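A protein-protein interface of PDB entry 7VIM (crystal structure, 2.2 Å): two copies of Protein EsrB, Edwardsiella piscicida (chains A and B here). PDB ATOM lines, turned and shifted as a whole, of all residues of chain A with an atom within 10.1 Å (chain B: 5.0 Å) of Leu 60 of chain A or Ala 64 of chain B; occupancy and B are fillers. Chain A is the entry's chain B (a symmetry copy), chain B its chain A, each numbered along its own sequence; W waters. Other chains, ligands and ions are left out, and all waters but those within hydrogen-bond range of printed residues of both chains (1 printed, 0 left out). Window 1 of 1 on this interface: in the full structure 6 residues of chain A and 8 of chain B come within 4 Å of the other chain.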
ATOM      1  N   MET A   4      32.710 -13.576  19.175  1.00  0.00           N
ATOM      2  CA  MET A   4      33.169 -12.836  20.346  1.00  0.00           C
ATOM      3  C   MET A   4      32.038 -12.649  21.358  1.00  0.00           C
ATOM      4  O   MET A   4      32.052 -11.706  22.148  1.00  0.00           O
ATOM      5  CB  MET A   4      33.748 -11.478  19.927  1.00  0.00           C
ATOM      6  CG  MET A   4      34.849 -10.933  20.852  1.00  0.00           C
ATOM      7  SD  MET A   4      36.426 -11.832  20.790  1.00  0.00           S
ATOM      8  CE  MET A   4      36.292 -12.914  22.217  1.00  0.00           C
ATOM      9  N   ALA A   5      31.060 -13.550  21.321  1.00  0.00           N
ATOM     10  CA  ALA A   5      29.961 -13.562  22.290  1.00  0.00           C
ATOM     11  C   ALA A   5      29.758 -14.973  22.835  1.00  0.00           C
ATOM     12  O   ALA A   5      29.818 -15.949  22.080  1.00  0.00           O
ATOM     13  CB  ALA A   5      28.671 -13.043  21.664  1.00  0.00           C
ATOM     14  N   GLU A   7      27.684 -17.746  25.750  1.00  0.00           N
ATOM     15  CA  GLU A   7      26.383 -18.004  26.348  1.00  0.00           C
ATOM     16  C   GLU A   7      26.418 -19.175  27.328  1.00  0.00           C
ATOM     17  O   GLU A   7      27.190 -20.117  27.136  1.00  0.00           O
ATOM     18  CB  GLU A   7      25.389 -18.292  25.226  1.00  0.00           C
ATOM     19  CG  GLU A   7      24.147 -17.417  25.233  1.00  0.00           C
ATOM     20  CD  GLU A   7      24.468 -15.927  25.141  1.00  0.00           C
ATOM     21  OE1 GLU A   7      25.167 -15.531  24.176  1.00  0.00           O
ATOM     22  OE2 GLU A   7      24.026 -15.158  26.039  1.00  0.00           O
ATOM     23  N   LEU A  52      18.527 -21.859  24.087  1.00  0.00           N
ATOM     24  CA  LEU A  52      18.767 -22.257  22.674  1.00  0.00           C
ATOM     25  C   LEU A  52      18.724 -20.998  21.800  1.00  0.00           C
ATOM     26  O   LEU A  52      19.621 -20.838  20.953  1.00  0.00           O
ATOM     27  CB  LEU A  52      17.703 -23.272  22.246  1.00  0.00           C
ATOM     28  CG  LEU A  52      17.867 -24.676  22.827  1.00  0.00           C
ATOM     29  CD1 LEU A  52      16.901 -25.651  22.172  1.00  0.00           C
ATOM     30  CD2 LEU A  52      19.299 -25.162  22.679  1.00  0.00           C
ATOM     31  N   ASP A  53      17.715 -20.147  22.008  1.00  0.00           N
ATOM     32  CA  ASP A  53      17.592 -18.891  21.255  1.00  0.00           C
ATOM     33  C   ASP A  53      18.848 -18.035  21.431  1.00  0.00           C
ATOM     34  O   ASP A  53      19.384 -17.495  20.454  1.00  0.00           O
ATOM     35  CB  ASP A  53      16.344 -18.063  21.623  1.00  0.00           C
ATOM     36  CG  ASP A  53      15.023 -18.755  21.235  1.00  0.00           C
ATOM     37  OD1 ASP A  53      15.001 -19.652  20.349  1.00  0.00           O
ATOM     38  OD2 ASP A  53      13.988 -18.390  21.829  1.00  0.00           O
ATOM     39  N   ALA A  54      19.316 -17.926  22.666  1.00  0.00           N
ATOM     40  CA  ALA A  54      20.474 -17.090  22.927  1.00  0.00           C
ATOM     41  C   ALA A  54      21.732 -17.676  22.293  1.00  0.00           C
ATOM     42  O   ALA A  54      22.524 -16.928  21.734  1.00  0.00           O
ATOM     43  CB  ALA A  54      20.668 -16.869  24.419  1.00  0.00           C
ATOM     44  N   HIS A  55      21.911 -18.998  22.377  1.00  0.00           N
ATOM     45  CA  HIS A  55      23.027 -19.652  21.688  1.00  0.00           C
ATOM     46  C   HIS A  55      22.951 -19.361  20.201  1.00  0.00           C
ATOM     47  O   HIS A  55      23.935 -19.004  19.565  1.00  0.00           O
ATOM     48  CB  HIS A  55      22.992 -21.169  21.884  1.00  0.00           C
ATOM     49  CG  HIS A  55      23.341 -21.607  23.270  1.00  0.00           C
ATOM     50  ND1 HIS A  55      23.055 -22.868  23.753  1.00  0.00           N
ATOM     51  CD2 HIS A  55      23.950 -20.947  24.282  1.00  0.00           C
ATOM     52  CE1 HIS A  55      23.471 -22.960  25.005  1.00  0.00           C
ATOM     53  NE2 HIS A  55      24.021 -21.809  25.348  1.00  0.00           N
ATOM     54  N   ASN A  56      21.754 -19.508  19.646  1.00  0.00           N
ATOM     55  CA  ASN A  56      21.577 -19.282  18.235  1.00  0.00           C
ATOM     56  C   ASN A  56      21.781 -17.834  17.809  1.00  0.00           C
ATOM     57  O   ASN A  56      22.274 -17.587  16.706  1.00  0.00           O
ATOM     58  CB  ASN A  56      20.217 -19.808  17.780  1.00  0.00           C
ATOM     59  CG  ASN A  56      20.155 -21.313  17.796  1.00  0.00           C
ATOM     60  OD1 ASN A  56      21.189 -21.970  17.751  1.00  0.00           O
ATOM     61  ND2 ASN A  56      18.954 -21.869  17.877  1.00  0.00           N
ATOM     62  N   ALA A  57      21.407 -16.885  18.673  1.00  0.00           N
ATOM     63  CA  ALA A  57      21.509 -15.469  18.323  1.00  0.00           C
ATOM     64  C   ALA A  57      22.968 -15.050  18.382  1.00  0.00           C
ATOM     65  O   ALA A  57      23.413 -14.224  17.606  1.00  0.00           O
ATOM     66  CB  ALA A  57      20.658 -14.578  19.262  1.00  0.00           C
ATOM     67  N   ALA A  58      23.701 -15.622  19.324  1.00  0.00           N
ATOM     68  CA  ALA A  58      25.107 -15.295  19.470  1.00  0.00           C
ATOM     69  C   ALA A  58      25.905 -15.863  18.291  1.00  0.00           C
ATOM     70  O   ALA A  58      26.786 -15.195  17.757  1.00  0.00           O
ATOM     71  CB  ALA A  58      25.656 -15.831  20.811  1.00  0.00           C
ATOM     72  N   GLU A  59      25.566 -17.083  17.886  1.00  0.00           N
ATOM     73  CA  GLU A  59      26.195 -17.722  16.722  1.00  0.00           C
ATOM     74  C   GLU A  59      26.043 -16.887  15.431  1.00  0.00           C
ATOM     75  O   GLU A  59      27.030 -16.637  14.700  1.00  0.00           O
ATOM     76  CB  GLU A  59      25.657 -19.157  16.551  1.00  0.00           C
ATOM     77  CG  GLU A  59      26.101 -19.902  15.276  1.00  0.00           C
ATOM     78  CD  GLU A  59      27.539 -20.442  15.331  1.00  0.00           C
ATOM     79  OE1 GLU A  59      28.249 -20.189  16.340  1.00  0.00           O
ATOM     80  OE2 GLU A  59      27.947 -21.136  14.360  1.00  0.00           O
ATOM     81  N   LEU A  60      24.824 -16.419  15.175  1.00  0.00           N
ATOM     82  CA  LEU A  60      24.570 -15.592  14.008  1.00  0.00           C
ATOM     83  C   LEU A  60      25.257 -14.229  14.089  1.00  0.00           C
ATOM     84  O   LEU A  60      25.773 -13.720  13.090  1.00  0.00           O
ATOM     85  CB  LEU A  60      23.075 -15.390  13.793  1.00  0.00           C
ATOM     86  CG  LEU A  60      22.284 -16.647  13.466  1.00  0.00           C
ATOM     87  CD1 LEU A  60      20.827 -16.274  13.163  1.00  0.00           C
ATOM     88  CD2 LEU A  60      22.939 -17.377  12.298  1.00  0.00           C
ATOM     89  N   SER A  61      25.236 -13.635  15.271  1.00  0.00           N
ATOM     90  CA  SER A  61      25.943 -12.378  15.503  1.00  0.00           C
ATOM     91  C   SER A  61      27.455 -12.531  15.326  1.00  0.00           C
ATOM     92  O   SER A  61      28.084 -11.695  14.700  1.00  0.00           O
ATOM     93  CB  SER A  61      25.631 -11.815  16.890  1.00  0.00           C
ATOM     94  OG  SER A  61      24.276 -11.420  16.946  1.00  0.00           O
ATOM     95  N   ASN A  62      28.027 -13.597  15.877  1.00  0.00           N
ATOM     96  CA  ASN A  62      29.452 -13.875  15.671  1.00  0.00           C
ATOM     97  C   ASN A  62      29.811 -13.941  14.186  1.00  0.00           C
ATOM     98  O   ASN A  62      30.767 -13.303  13.737  1.00  0.00           O
ATOM     99  CB  ASN A  62      29.890 -15.170  16.377  1.00  0.00           C
ATOM    100  CG  ASN A  62      29.869 -15.045  17.879  1.00  0.00           C
ATOM    101  OD1 ASN A  62      29.950 -13.940  18.414  1.00  0.00           O
ATOM    102  ND2 ASN A  62      29.738 -16.176  18.574  1.00  0.00           N
ATOM    103  N   TRP A  63      29.022 -14.695  13.427  1.00  0.00           N
ATOM    104  CA  TRP A  63      29.254 -14.806  11.996  1.00  0.00           C
ATOM    105  C   TRP A  63      29.064 -13.485  11.264  1.00  0.00           C
ATOM    106  O   TRP A  63      29.790 -13.203  10.318  1.00  0.00           O
ATOM    107  CB  TRP A  63      28.402 -15.913  11.376  1.00  0.00           C
ATOM    108  CG  TRP A  63      29.000 -17.265  11.605  1.00  0.00           C
ATOM    109  CD1 TRP A  63      28.464 -18.288  12.322  1.00  0.00           C
ATOM    110  CD2 TRP A  63      30.275 -17.725  11.142  1.00  0.00           C
ATOM    111  NE1 TRP A  63      29.313 -19.360  12.329  1.00  0.00           N
ATOM    112  CE2 TRP A  63      30.434 -19.044  11.612  1.00  0.00           C
ATOM    113  CE3 TRP A  63      31.296 -17.148  10.370  1.00  0.00           C
ATOM    114  CZ2 TRP A  63      31.569 -19.807  11.327  1.00  0.00           C
ATOM    115  CZ3 TRP A  63      32.430 -17.901  10.098  1.00  0.00           C
ATOM    116  CH2 TRP A  63      32.554 -19.220  10.574  1.00  0.00           C
ATOM    117  N   ALA A  64      28.102 -12.673  11.702  1.00  0.00           N
ATOM    118  CA  ALA A  64      27.882 -11.382  11.067  1.00  0.00           C
ATOM    119  C   ALA A  64      29.104 -10.502  11.285  1.00  0.00           C
ATOM    120  O   ALA A  64      29.533  -9.789  10.373  1.00  0.00           O
ATOM    121  CB  ALA A  64      26.635 -10.696  11.614  1.00  0.00           C
ATOM    122  N   ARG A  65      29.664 -10.565  12.491  1.00  0.00           N
ATOM    123  CA  ARG A  65      30.897  -9.838  12.780  1.00  0.00           C
ATOM    124  C   ARG A  65      32.067 -10.366  11.935  1.00  0.00           C
ATOM    125  O   ARG A  65      32.741  -9.581  11.286  1.00  0.00           O
ATOM    126  CB  ARG A  65      31.234  -9.867  14.275  1.00  0.00           C
ATOM    127  CG  ARG A  65      30.395  -8.901  15.122  1.00  0.00           C
ATOM    128  CD  ARG A  65      30.874  -8.816  16.580  1.00  0.00           C
ATOM    129  NE  ARG A  65      30.398  -9.929  17.402  1.00  0.00           N
ATOM    130  CZ  ARG A  65      29.205  -9.969  18.000  1.00  0.00           C
ATOM    131  NH1 ARG A  65      28.350  -8.963  17.863  1.00  0.00           N
ATOM    132  NH2 ARG A  65      28.863 -11.022  18.736  1.00  0.00           N
ATOM    133  N   ARG A  66      32.274 -11.685  11.927  1.00  0.00           N
ATOM    134  CA  ARG A  66      33.352 -12.306  11.142  1.00  0.00           C
ATOM    135  C   ARG A  66      33.283 -12.018   9.644  1.00  0.00           C
ATOM    136  O   ARG A  66      34.322 -11.972   8.960  1.00  0.00           O
ATOM    137  CB  ARG A  66      33.389 -13.824  11.354  1.00  0.00           C
ATOM    138  CG  ARG A  66      33.804 -14.268  12.754  1.00  0.00           C
ATOM    139  CD  ARG A  66      33.581 -15.769  12.894  1.00  0.00           C
ATOM    140  NE  ARG A  66      33.854 -16.269  14.236  1.00  0.00           N
ATOM    141  CZ  ARG A  66      33.111 -17.176  14.874  1.00  0.00           C
ATOM    142  NH1 ARG A  66      32.027 -17.695  14.297  1.00  0.00           N
ATOM    143  NH2 ARG A  66      33.446 -17.568  16.100  1.00  0.00           N
ATOM    144  N   LEU A  67      32.068 -11.835   9.125  1.00  0.00           N
ATOM    145  CA  LEU A  67      31.903 -11.612   7.698  1.00  0.00           C
ATOM    146  C   LEU A  67      31.717 -10.146   7.333  1.00  0.00           C
ATOM    147  O   LEU A  67      31.529  -9.817   6.165  1.00  0.00           O
ATOM    148  CB  LEU A  67      30.750 -12.452   7.152  1.00  0.00           C
ATOM    149  CG  LEU A  67      30.916 -13.954   7.332  1.00  0.00           C
ATOM    150  CD1 LEU A  67      29.683 -14.675   6.846  1.00  0.00           C
ATOM    151  CD2 LEU A  67      32.144 -14.430   6.559  1.00  0.00           C
ATOM    152  N   GLY A  68      31.766  -9.272   8.335  1.00  0.00           N
ATOM    153  CA  GLY A  68      31.649  -7.843   8.102  1.00  0.00           C
ATOM    154  C   GLY A  68      30.270  -7.353   7.692  1.00  0.00           C
ATOM    155  O   GLY A  68      30.155  -6.361   6.970  1.00  0.00           O
ATOM    156  N   VAL A  69      29.206  -8.024   8.130  1.00  0.00           N
ATOM    157  CA  VAL A  69      27.864  -7.584   7.724  1.00  0.00           C
ATOM    158  C   VAL A  69      27.052  -6.855   8.809  1.00  0.00           C
ATOM    159  O   VAL A  69      27.163  -7.172   9.991  1.00  0.00           O
ATOM    160  CB  VAL A  69      27.047  -8.721   7.061  1.00  0.00           C
ATOM    161  CG1 VAL A  69      27.431  -8.847   5.603  1.00  0.00           C
ATOM    162  CG2 VAL A  69      27.274 -10.026   7.763  1.00  0.00           C
ATOM    163  N   LEU A  70      26.259  -5.867   8.376  1.00  0.00           N
ATOM    164  CA  LEU A  70      25.363  -5.058   9.237  1.00  0.00           C
ATOM    165  C   LEU A  70      26.047  -4.445  10.449  1.00  0.00           C
ATOM    166  O   LEU A  70      26.818  -3.497  10.304  1.00  0.00           O
ATOM    167  CB  LEU A  70      24.111  -5.835   9.664  1.00  0.00           C
ATOM    168  CG  LEU A  70      22.907  -5.740   8.723  1.00  0.00           C
ATOM    169  CD1 LEU A  70      21.870  -6.822   9.038  1.00  0.00           C
ATOM    170  CD2 LEU A  70      22.287  -4.339   8.806  1.00  0.00           C
ATOM    171  N   LEU B  60      22.340 -14.776   6.402  1.00  0.00           N
ATOM    172  CA  LEU B  60      22.253 -14.678   7.855  1.00  0.00           C
ATOM    173  C   LEU B  60      20.857 -14.247   8.320  1.00  0.00           C
ATOM    174  O   LEU B  60      20.341 -14.740   9.334  1.00  0.00           O
ATOM    175  CB  LEU B  60      23.302 -13.704   8.394  1.00  0.00           C
ATOM    176  CG  LEU B  60      24.747 -14.192   8.195  1.00  0.00           C
ATOM    177  CD1 LEU B  60      25.757 -13.160   8.677  1.00  0.00           C
ATOM    178  CD2 LEU B  60      24.969 -15.490   8.927  1.00  0.00           C
ATOM    179  N   SER B  61      20.269 -13.338   7.550  1.00  0.00           N
ATOM    180  CA  SER B  61      18.913 -12.855   7.765  1.00  0.00           C
ATOM    181  C   SER B  61      17.888 -13.980   7.632  1.00  0.00           C
ATOM    182  O   SER B  61      16.963 -14.086   8.434  1.00  0.00           O
ATOM    183  CB  SER B  61      18.613 -11.712   6.772  1.00  0.00           C
ATOM    184  OG  SER B  61      17.241 -11.378   6.752  1.00  0.00           O
ATOM    185  N   ASN B  62      18.055 -14.818   6.619  1.00  0.00           N
ATOM    186  CA  ASN B  62      17.178 -15.971   6.445  1.00  0.00           C
ATOM    187  C   ASN B  62      17.349 -16.993   7.558  1.00  0.00           C
ATOM    188  O   ASN B  62      16.374 -17.590   7.999  1.00  0.00           O
ATOM    189  CB  ASN B  62      17.389 -16.627   5.081  1.00  0.00           C
ATOM    190  CG  ASN B  62      16.785 -15.815   3.948  1.00  0.00           C
ATOM    191  OD1 ASN B  62      15.929 -14.964   4.176  1.00  0.00           O
ATOM    192  ND2 ASN B  62      17.236 -16.071   2.721  1.00  0.00           N
ATOM    193  N   TRP B  63      18.581 -17.178   8.026  1.00  0.00           N
ATOM    194  CA  TRP B  63      18.799 -18.039   9.184  1.00  0.00           C
ATOM    195  C   TRP B  63      18.192 -17.483  10.474  1.00  0.00           C
ATOM    196  O   TRP B  63      17.644 -18.236  11.268  1.00  0.00           O
ATOM    197  CB  TRP B  63      20.279 -18.403   9.370  1.00  0.00           C
ATOM    198  CG  TRP B  63      20.718 -19.472   8.424  1.00  0.00           C
ATOM    199  CD1 TRP B  63      21.581 -19.334   7.383  1.00  0.00           C
ATOM    200  CD2 TRP B  63      20.281 -20.838   8.407  1.00  0.00           C
ATOM    201  NE1 TRP B  63      21.730 -20.528   6.734  1.00  0.00           N
ATOM    202  CE2 TRP B  63      20.939 -21.467   7.333  1.00  0.00           C
ATOM    203  CE3 TRP B  63      19.408 -21.591   9.204  1.00  0.00           C
ATOM    204  CZ2 TRP B  63      20.754 -22.819   7.032  1.00  0.00           C
ATOM    205  CZ3 TRP B  63      19.218 -22.928   8.900  1.00  0.00           C
ATOM    206  CH2 TRP B  63      19.890 -23.529   7.825  1.00  0.00           C
ATOM    207  N   ALA B  64      18.280 -16.173  10.675  1.00  0.00           N
ATOM    208  CA  ALA B  64      17.662 -15.562  11.843  1.00  0.00           C
ATOM    209  C   ALA B  64      16.162 -15.839  11.866  1.00  0.00           C
ATOM    210  O   ALA B  64      15.597 -16.148  12.922  1.00  0.00           O
ATOM    211  CB  ALA B  64      17.931 -14.061  11.892  1.00  0.00           C
ATOM    212  N   ARG B  65      15.529 -15.762  10.701  1.00  0.00           N
ATOM    213  CA  ARG B  65      14.100 -16.041  10.600  1.00  0.00           C
ATOM    214  C   ARG B  65      13.787 -17.516  10.830  1.00  0.00           C
ATOM    215  O   ARG B  65      12.829 -17.833  11.507  1.00  0.00           O
ATOM    216  CB  ARG B  65      13.535 -15.581   9.251  1.00  0.00           C
ATOM    217  CG  ARG B  65      13.743 -14.107   8.983  1.00  0.00           C
ATOM    218  CD  ARG B  65      12.668 -13.581   8.049  1.00  0.00           C
ATOM    219  NE  ARG B  65      13.249 -12.873   6.918  1.00  0.00           N
ATOM    220  CZ  ARG B  65      12.584 -12.563   5.812  1.00  0.00           C
ATOM    221  NH1 ARG B  65      11.305 -12.906   5.688  1.00  0.00           N
ATOM    222  NH2 ARG B  65      13.201 -11.919   4.829  1.00  0.00           N
ATOM    223  N   ARG B  66      14.587 -18.405  10.254  1.00  0.00           N
ATOM    224  CA  ARG B  66      14.433 -19.843  10.503  1.00  0.00           C
ATOM    225  C   ARG B  66      14.624 -20.258  11.950  1.00  0.00           C
ATOM    226  O   ARG B  66      13.989 -21.211  12.404  1.00  0.00           O
ATOM    227  CB  ARG B  66      15.396 -20.659   9.643  1.00  0.00           C
ATOM    228  CG  ARG B  66      15.012 -20.677   8.194  1.00  0.00           C
ATOM    229  CD  ARG B  66      16.008 -21.455   7.363  1.00  0.00           C
ATOM    230  NE  ARG B  66      16.293 -20.753   6.126  1.00  0.00           N
ATOM    231  CZ  ARG B  66      16.758 -21.331   5.026  1.00  0.00           C
ATOM    232  NH1 ARG B  66      16.984 -22.642   5.007  1.00  0.00           N
ATOM    233  NH2 ARG B  66      16.994 -20.593   3.946  1.00  0.00           N
ATOM    234  N   LEU B  67      15.524 -19.573  12.657  1.00  0.00           N
ATOM    235  CA  LEU B  67      15.800 -19.893  14.053  1.00  0.00           C
ATOM    236  C   LEU B  67      14.919 -19.078  14.996  1.00  0.00           C
ATOM    237  O   LEU B  67      14.988 -19.239  16.213  1.00  0.00           O
ATOM    238  CB  LEU B  67      17.286 -19.673  14.392  1.00  0.00           C
ATOM    239  CG  LEU B  67      18.316 -20.404  13.517  1.00  0.00           C
ATOM    240  CD1 LEU B  67      19.731 -20.225  14.069  1.00  0.00           C
ATOM    241  CD2 LEU B  67      17.979 -21.870  13.416  1.00  0.00           C
ATOM    242  N   GLY B  68      14.100 -18.195  14.425  1.00  0.00           N
ATOM    243  CA  GLY B  68      13.232 -17.325  15.208  1.00  0.00           C
ATOM    244  C   GLY B  68      13.948 -16.433  16.209  1.00  0.00           C
ATOM    245  O   GLY B  68      13.476 -16.253  17.317  1.00  0.00           O
ATOM    246  N   VAL B  69      15.102 -15.882  15.826  1.00  0.00           N
ATOM    247  CA  VAL B  69      15.837 -14.971  16.703  1.00  0.00           C
ATOM    248  C   VAL B  69      16.095 -13.598  16.080  1.00  0.00           C
ATOM    249  O   VAL B  69      15.927 -13.401  14.888  1.00  0.00           O
ATOM    250  CB  VAL B  69      17.212 -15.549  17.152  1.00  0.00           C
ATOM    251  CG1 VAL B  69      17.020 -16.808  17.950  1.00  0.00           C
ATOM    252  CG2 VAL B  69      18.129 -15.758  15.942  1.00  0.00           C
ATOM    253  N   LEU B  70      16.508 -12.666  16.932  1.00  0.00           N
ATOM    254  CA  LEU B  70      16.949 -11.333  16.534  1.00  0.00           C
ATOM    255  C   LEU B  70      15.830 -10.488  15.904  1.00  0.00           C
ATOM    256  O   LEU B  70      15.969  -9.988  14.782  1.00  0.00           O
ATOM    257  CB  LEU B  70      18.183 -11.432  15.624  1.00  0.00           C
ATOM    258  CG  LEU B  70      19.428 -12.099  16.247  1.00  0.00           C
ATOM    259  CD1 LEU B  70      20.461 -12.429  15.186  1.00  0.00           C
ATOM    260  CD2 LEU B  70      20.062 -11.223  17.319  1.00  0.00           C
HETATM  261  O   HOH W   1      16.582 -20.357  18.128  1.00  0.00           O
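The backbone carbonyl oxygen of Ala 64 of chain B sits at hydrogen-bond distance from the backbone NH of Val 69 of chain B, at 3.0 Å.
The side-chain amide nitrogen (ND2) of Asn 56 of chain A lies close to the backbone carbonyl oxygen (O) of Leu 52 of chain A, at 3.3 Å.
O of Ala 57 of chain A sits at hydrogen-bond distance from OG of Ser 61 of chain A, at 3.0 Å.
The backbone carbonyl oxygen of Ala 64 of chain A lies within hydrogen-bond range of the backbone NH of Val 69 of chain A (2.9 Å).
O of Asp 53 of chain A touches CG1 of Val 69 of chain B (3.5 Å).
CB of Asn 56 of chain A touches CD1 of Leu 67 of chain B, 3.8 Å away.
CB of Ala 57 of chain A touches CD2 of Leu 70 of chain B (3.9 Å).
Leu 60 of chain A touches Trp 63 of chain B (CD1 to C, 3.95 Å).
Leu 60 of chain A touches Ala 64 of chain B (CD1 to CA, 3.5 Å).
Val 69 of chain B touches Leu 60 of chain A (CG2 to CD1, 3.9 Å).
CD1 of Leu 60 of chain B touches CA of Ala 64 of chain A, at 3.7 Å.
Val 69 of chain A touches Leu 60 of chain B.
Water W1 lies within hydrogen-bond range of O of Leu 67 of chain B (2.7 Å), OD1 of Asp 53 of chain A (2.8 Å) and ND2 of Asn 56 of chain A (2.8 Å).
Leu 60 of chain A touches Trp 63 of chain B, but with the chains exchanged Trp 63 of chain A does not touch Leu 60 of chain B (4.2 Å).
Leu 60 of chain A touches Ala 64 of chain B, and with the chains exchanged Ala 64 of chain A touches Leu 60 of chain B.
Leu 60 of chain A touches Val 69 of chain B, and with the chains exchanged Val 69 of chain A touches Leu 60 of chain B.
Hydrophobic or aromatic side chains of chain B within 4 Å of the printed part of chain A: Leu 60, Ala 64, Leu 67, Val 69 and Leu 70.
Of the 22 printed residues of chain A, 6 touch a printed residue of chain B.
Printed residues of chain A that touch a printed residue of chain B: Asp 53, Asn 56, Ala 57, Leu 60, Ala 64 and Val 69.
Among the printed residues, no Asp or Glu carboxylate lies within 4 Å of a Lys or Arg side-chain nitrogen of the other chain.
Leu 60 of chain A touches just these residues of chain B: Trp 63 (3.95 Å), Ala 64 (3.5 Å) and Val 69 (3.9 Å).
Ala 64 of chain B touches just one residue of chain A: Leu 60.
No residue of chain A comes within 4 Å of Ser 61 of chain B.
No residue of chain A comes within 4 Å of Gly 68 of chain B.
Of chain A, only Asp 53 (3.5 Å) and Leu 60 (3.9 Å) come within 4 Å of Val 69 of chain B.
Of the printed residues of chain A, Leu 60 of chain B touches Ala 64 (3.7 Å) and Val 69 (3.6 Å).
Of the printed residues of chain B, Ala 57 of chain A touches Leu 70 (3.9 Å).
Of the printed residues of chain B, Val 69 of chain A touches Leu 60 (3.6 Å).
Of the printed residues of chain B, Asn 56 of chain A touches Leu 67.
Of the printed residues of chain B, Asp 53 of chain A touches Val 69 (3.5 Å).
The nearest residue of chain B that does not touch Leu 60 of chain A is Leu 60 of chain B (4.2 Å).
The nearest residue of chain A that does not touch Ala 64 of chain B is Asn 56 of chain A (7.0 Å).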
